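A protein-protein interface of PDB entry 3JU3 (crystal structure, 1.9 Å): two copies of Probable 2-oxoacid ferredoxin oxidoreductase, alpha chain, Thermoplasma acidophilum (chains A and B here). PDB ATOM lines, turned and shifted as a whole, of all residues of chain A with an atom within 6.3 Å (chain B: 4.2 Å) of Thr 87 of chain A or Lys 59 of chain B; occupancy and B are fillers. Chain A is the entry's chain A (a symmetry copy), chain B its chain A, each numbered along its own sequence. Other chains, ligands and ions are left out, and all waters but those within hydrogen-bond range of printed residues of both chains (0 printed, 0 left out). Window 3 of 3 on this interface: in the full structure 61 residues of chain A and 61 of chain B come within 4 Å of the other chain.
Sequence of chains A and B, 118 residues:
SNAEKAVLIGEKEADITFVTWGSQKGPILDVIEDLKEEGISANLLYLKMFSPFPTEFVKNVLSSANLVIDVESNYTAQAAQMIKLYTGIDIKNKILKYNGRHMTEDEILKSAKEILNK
The side-chain hydroxyl (OG) of Ser 63 of chain B lies close to the backbone carbonyl oxygen (O) of Lys 59 of chain B (3.3 Å).
O of Ile 83 of chain A sits at hydrogen-bond distance from OG1 of Thr 87 of chain A (2.5 Å).
The backbone NH (N) of Ile 89 of chain A lies within hydrogen-bond range of the side-chain hydroxyl (OG1) of Thr 87 of chain A (3.1 Å).
Among the printed residues, merely in contact across the chains: Ile 83 of chain A with Leu 62 of chain B, Tyr 86 of chain A with Thr 55 of chain B, Thr 87 of chain A with Thr 55 of chain B, Thr 87 of chain A with Lys 59 of chain B, Ile 89 of chain A with Lys 59 of chain B and Ile 89 of chain A with Leu 62 of chain B.
Of the printed residues of chain B, Thr 87 of chain A touches Thr 55 and Lys 59.
Lys 59 of chain B touches two residues of chain A.
Printed residues of chain B within 4 Å of Ile 83 of chain A: Leu 62 (3.7 Å).
Printed residues of chain A within 4 Å of Thr 55 of chain B: Tyr 86 (3.4 Å) and Thr 87 (3.7 Å).
Of the printed residues of chain A, Leu 62 of chain B touches Ile 83 (3.7 Å) and Ile 89 (3.9 Å).
Printed residues of chain B within 4 Å of Tyr 86 of chain A: Thr 55 (3.4 Å).
Of the printed residues of chain B, Ile 89 of chain A touches Lys 59 and Leu 62.
The nearest printed residue of chain B that does not touch Thr 87 of chain A is Val 58 of chain B (4.2 Å).
The nearest residue of chain A that does not touch Lys 59 of chain B is Tyr 86 of chain A (5.8 Å).
The nearest printed residue of chain B that does not touch Tyr 86 of chain A is Lys 59 of chain B (5.8 Å).
Hydrophobic or aromatic side chains of chain A that line the printed part of chain B: Ile 83, Tyr 86 and Ile 89.
Hydrophobic or aromatic side chains of chain B that line the printed part of chain A: Leu 62.
Along chain B the printed residues that touch a printed residue of chain A span positions 55 to 62.
Among the printed residues, 6 pairs touch across the chains.
No position is printed for both chains.
Of the 6 pairs that touch across the chains among the printed residues, none has its exchanged pair printed and touching as well.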
ATOM      1  N   MET A  82      -3.889  28.916  15.838  1.00  0.00           N
ATOM      2  CA  MET A  82      -4.411  29.563  17.038  1.00  0.00           C
ATOM      3  C   MET A  82      -5.084  28.558  17.985  1.00  0.00           C
ATOM      4  O   MET A  82      -5.075  28.761  19.183  1.00  0.00           O
ATOM      5  CB  MET A  82      -5.296  30.760  16.674  1.00  0.00           C
ATOM      6  CG  MET A  82      -6.753  30.486  16.651  1.00  0.00           C
ATOM      7  SD  MET A  82      -7.753  32.022  15.988  1.00  0.00           S
ATOM      8  CE  MET A  82      -8.418  31.183  14.371  1.00  0.00           C
ATOM      9  N   ILE A  83      -5.640  27.477  17.441  1.00  0.00           N
ATOM     10  CA  ILE A  83      -6.256  26.406  18.229  1.00  0.00           C
ATOM     11  C   ILE A  83      -5.185  25.729  19.076  1.00  0.00           C
ATOM     12  O   ILE A  83      -5.413  25.451  20.258  1.00  0.00           O
ATOM     13  CB  ILE A  83      -6.967  25.381  17.331  1.00  0.00           C
ATOM     14  CG1 ILE A  83      -8.204  26.023  16.689  1.00  0.00           C
ATOM     15  CG2 ILE A  83      -7.372  24.083  18.113  1.00  0.00           C
ATOM     16  CD1 ILE A  83      -8.916  25.141  15.659  1.00  0.00           C
ATOM     17  N   LYS A  84      -4.040  25.448  18.462  1.00  0.00           N
ATOM     18  CA  LYS A  84      -2.911  24.885  19.167  1.00  0.00           C
ATOM     19  C   LYS A  84      -2.422  25.811  20.271  1.00  0.00           C
ATOM     20  O   LYS A  84      -2.111  25.339  21.368  1.00  0.00           O
ATOM     21  CB  LYS A  84      -1.745  24.561  18.212  1.00  0.00           C
ATOM     22  CG  LYS A  84      -0.574  23.904  18.941  1.00  0.00           C
ATOM     23  CD  LYS A  84       0.392  23.243  17.980  1.00  0.00           C
ATOM     24  CE  LYS A  84       1.501  24.182  17.545  1.00  0.00           C
ATOM     25  NZ  LYS A  84       2.397  23.510  16.566  1.00  0.00           N
ATOM     26  N   LEU A  85      -2.350  27.109  19.957  1.00  0.00           N
ATOM     27  CA  LEU A  85      -1.859  28.120  20.888  1.00  0.00           C
ATOM     28  C   LEU A  85      -2.732  28.076  22.128  1.00  0.00           C
ATOM     29  O   LEU A  85      -2.225  27.958  23.243  1.00  0.00           O
ATOM     30  CB  LEU A  85      -1.929  29.527  20.272  1.00  0.00           C
ATOM     31  CG  LEU A  85      -1.685  30.677  21.263  1.00  0.00           C
ATOM     32  CD1 LEU A  85      -0.213  30.671  21.694  1.00  0.00           C
ATOM     33  CD2 LEU A  85      -2.090  32.062  20.713  1.00  0.00           C
ATOM     34  N   TYR A  86      -4.048  28.169  21.924  1.00  0.00           N
ATOM     35  CA  TYR A  86      -4.954  28.270  23.046  1.00  0.00           C
ATOM     36  C   TYR A  86      -5.276  26.990  23.787  1.00  0.00           C
ATOM     37  O   TYR A  86      -5.426  27.032  25.007  1.00  0.00           O
ATOM     38  CB  TYR A  86      -6.244  28.982  22.683  1.00  0.00           C
ATOM     39  CG  TYR A  86      -6.090  30.427  22.385  1.00  0.00           C
ATOM     40  CD1 TYR A  86      -5.843  31.351  23.406  1.00  0.00           C
ATOM     41  CD2 TYR A  86      -6.212  30.894  21.087  1.00  0.00           C
ATOM     42  CE1 TYR A  86      -5.746  32.722  23.123  1.00  0.00           C
ATOM     43  CE2 TYR A  86      -6.109  32.282  20.785  1.00  0.00           C
ATOM     44  CZ  TYR A  86      -5.861  33.179  21.814  1.00  0.00           C
ATOM     45  OH  TYR A  86      -5.746  34.526  21.535  1.00  0.00           O
ATOM     46  N   THR A  87      -5.409  25.870  23.068  1.00  0.00           N
ATOM     47  CA  THR A  87      -5.924  24.623  23.644  1.00  0.00           C
ATOM     48  C   THR A  87      -4.903  23.512  23.752  1.00  0.00           C
ATOM     49  O   THR A  87      -5.149  22.521  24.437  1.00  0.00           O
ATOM     50  CB  THR A  87      -7.036  24.014  22.778  1.00  0.00           C
ATOM     51  OG1 THR A  87      -6.451  23.556  21.546  1.00  0.00           O
ATOM     52  CG2 THR A  87      -8.168  25.021  22.529  1.00  0.00           C
ATOM     53  N   GLY A  88      -3.782  23.648  23.050  1.00  0.00           N
ATOM     54  CA  GLY A  88      -2.777  22.619  23.038  1.00  0.00           C
ATOM     55  C   GLY A  88      -3.060  21.462  22.104  1.00  0.00           C
ATOM     56  O   GLY A  88      -2.229  20.573  21.981  1.00  0.00           O
ATOM     57  N   ILE A  89      -4.224  21.451  21.447  1.00  0.00           N
ATOM     58  CA  ILE A  89      -4.510  20.410  20.449  1.00  0.00           C
ATOM     59  C   ILE A  89      -3.817  20.751  19.139  1.00  0.00           C
ATOM     60  O   ILE A  89      -3.946  21.858  18.641  1.00  0.00           O
ATOM     61  CB  ILE A  89      -6.016  20.222  20.242  1.00  0.00           C
ATOM     62  CG1 ILE A  89      -6.618  19.612  21.497  1.00  0.00           C
ATOM     63  CG2 ILE A  89      -6.317  19.344  19.014  1.00  0.00           C
ATOM     64  CD1 ILE A  89      -8.010  20.086  21.760  1.00  0.00           C
ATOM     65  N   ASP A  90      -3.049  19.812  18.605  1.00  0.00           N
ATOM     66  CA  ASP A  90      -2.468  20.001  17.285  1.00  0.00           C
ATOM     67  C   ASP A  90      -3.153  19.118  16.240  1.00  0.00           C
ATOM     68  O   ASP A  90      -2.858  17.915  16.105  1.00  0.00           O
ATOM     69  CB  ASP A  90      -0.940  19.808  17.270  1.00  0.00           C
ATOM     70  CG  ASP A  90      -0.282  20.438  16.027  1.00  0.00           C
ATOM     71  OD1 ASP A  90      -0.938  21.299  15.381  1.00  0.00           O
ATOM     72  OD2 ASP A  90       0.862  20.077  15.687  1.00  0.00           O
ATOM     73  N   THR B  55     -11.549  28.938  24.346  1.00  0.00           N
ATOM     74  CA  THR B  55     -10.626  27.841  24.661  1.00  0.00           C
ATOM     75  C   THR B  55     -11.360  26.578  25.114  1.00  0.00           C
ATOM     76  O   THR B  55     -11.194  25.519  24.512  1.00  0.00           O
ATOM     77  CB  THR B  55      -9.596  28.272  25.734  1.00  0.00           C
ATOM     78  OG1 THR B  55      -8.811  29.350  25.211  1.00  0.00           O
ATOM     79  CG2 THR B  55      -8.676  27.109  26.144  1.00  0.00           C
ATOM     80  N   GLU B  56     -12.181  26.698  26.156  1.00  0.00           N
ATOM     81  CA  GLU B  56     -12.856  25.527  26.735  1.00  0.00           C
ATOM     82  C   GLU B  56     -13.791  24.827  25.731  1.00  0.00           C
ATOM     83  O   GLU B  56     -13.784  23.614  25.617  1.00  0.00           O
ATOM     84  CB  GLU B  56     -13.631  25.924  28.005  1.00  0.00           C
ATOM     85  CG  GLU B  56     -14.291  24.726  28.693  1.00  0.00           C
ATOM     86  CD  GLU B  56     -14.936  25.073  30.030  1.00  0.00           C
ATOM     87  OE1 GLU B  56     -15.413  26.219  30.200  1.00  0.00           O
ATOM     88  OE2 GLU B  56     -14.974  24.178  30.908  1.00  0.00           O
ATOM     89  N   PHE B  57     -14.578  25.611  25.007  1.00  0.00           N
ATOM     90  CA  PHE B  57     -15.531  25.090  24.037  1.00  0.00           C
ATOM     91  C   PHE B  57     -14.827  24.330  22.917  1.00  0.00           C
ATOM     92  O   PHE B  57     -15.256  23.234  22.533  1.00  0.00           O
ATOM     93  CB  PHE B  57     -16.410  26.219  23.454  1.00  0.00           C
ATOM     94  CG  PHE B  57     -17.446  25.735  22.447  1.00  0.00           C
ATOM     95  CD1 PHE B  57     -18.754  25.432  22.843  1.00  0.00           C
ATOM     96  CD2 PHE B  57     -17.115  25.608  21.106  1.00  0.00           C
ATOM     97  CE1 PHE B  57     -19.716  24.965  21.887  1.00  0.00           C
ATOM     98  CE2 PHE B  57     -18.043  25.141  20.161  1.00  0.00           C
ATOM     99  CZ  PHE B  57     -19.333  24.823  20.531  1.00  0.00           C
ATOM    100  N   VAL B  58     -13.766  24.927  22.382  1.00  0.00           N
ATOM    101  CA  VAL B  58     -13.035  24.318  21.280  1.00  0.00           C
ATOM    102  C   VAL B  58     -12.339  23.080  21.801  1.00  0.00           C
ATOM    103  O   VAL B  58     -12.389  22.013  21.178  1.00  0.00           O
ATOM    104  CB  VAL B  58     -12.065  25.285  20.636  1.00  0.00           C
ATOM    105  CG1 VAL B  58     -11.177  24.565  19.607  1.00  0.00           C
ATOM    106  CG2 VAL B  58     -12.865  26.421  19.965  1.00  0.00           C
ATOM    107  N   LYS B  59     -11.717  23.220  22.962  1.00  0.00           N
ATOM    108  CA  LYS B  59     -11.022  22.091  23.559  1.00  0.00           C
ATOM    109  C   LYS B  59     -11.966  20.887  23.736  1.00  0.00           C
ATOM    110  O   LYS B  59     -11.594  19.781  23.371  1.00  0.00           O
ATOM    111  CB  LYS B  59     -10.333  22.493  24.885  1.00  0.00           C
ATOM    112  CG  LYS B  59      -9.104  21.679  25.263  1.00  0.00           C
ATOM    113  CD  LYS B  59      -8.408  22.265  26.484  1.00  0.00           C
ATOM    114  CE  LYS B  59      -7.485  21.245  27.108  1.00  0.00           C
ATOM    115  NZ  LYS B  59      -6.669  21.911  28.169  1.00  0.00           N
ATOM    116  N   ASN B  60     -13.164  21.097  24.273  1.00  0.00           N
ATOM    117  CA  ASN B  60     -14.085  19.967  24.512  1.00  0.00           C
ATOM    118  C   ASN B  60     -14.759  19.391  23.247  1.00  0.00           C
ATOM    119  O   ASN B  60     -15.176  18.241  23.236  1.00  0.00           O
ATOM    120  CB  ASN B  60     -15.130  20.328  25.575  1.00  0.00           C
ATOM    121  CG  ASN B  60     -14.505  20.823  26.872  1.00  0.00           C
ATOM    122  OD1 ASN B  60     -13.379  20.448  27.225  1.00  0.00           O
ATOM    123  ND2 ASN B  60     -15.237  21.668  27.595  1.00  0.00           N
ATOM    124  N   VAL B  61     -14.859  20.179  22.179  1.00  0.00           N
ATOM    125  CA  VAL B  61     -15.283  19.634  20.888  1.00  0.00           C
ATOM    126  C   VAL B  61     -14.184  18.783  20.256  1.00  0.00           C
ATOM    127  O   VAL B  61     -14.432  17.679  19.820  1.00  0.00           O
ATOM    128  CB  VAL B  61     -15.769  20.725  19.898  1.00  0.00           C
ATOM    129  CG1 VAL B  61     -15.933  20.131  18.481  1.00  0.00           C
ATOM    130  CG2 VAL B  61     -17.058  21.350  20.395  1.00  0.00           C
ATOM    131  N   LEU B  62     -12.960  19.279  20.236  1.00  0.00           N
ATOM    132  CA  LEU B  62     -11.922  18.609  19.462  1.00  0.00           C
ATOM    133  C   LEU B  62     -11.356  17.419  20.229  1.00  0.00           C
ATOM    134  O   LEU B  62     -10.908  16.415  19.629  1.00  0.00           O
ATOM    135  CB  LEU B  62     -10.819  19.589  19.068  1.00  0.00           C
ATOM    136  CG  LEU B  62     -11.208  20.711  18.090  1.00  0.00           C
ATOM    137  CD1 LEU B  62      -9.986  21.479  17.707  1.00  0.00           C
ATOM    138  CD2 LEU B  62     -11.919  20.200  16.834  1.00  0.00           C
ATOM    139  N   SER B  63     -11.447  17.491  21.558  1.00  0.00           N
ATOM    140  CA  SER B  63     -10.858  16.471  22.411  1.00  0.00           C
ATOM    141  C   SER B  63     -11.541  15.103  22.223  1.00  0.00           C
ATOM    142  O   SER B  63     -10.915  14.053  22.436  1.00  0.00           O
ATOM    143  CB  SER B  63     -10.945  16.917  23.874  1.00  0.00           C
ATOM    144  OG  SER B  63     -12.273  16.739  24.361  1.00  0.00           O
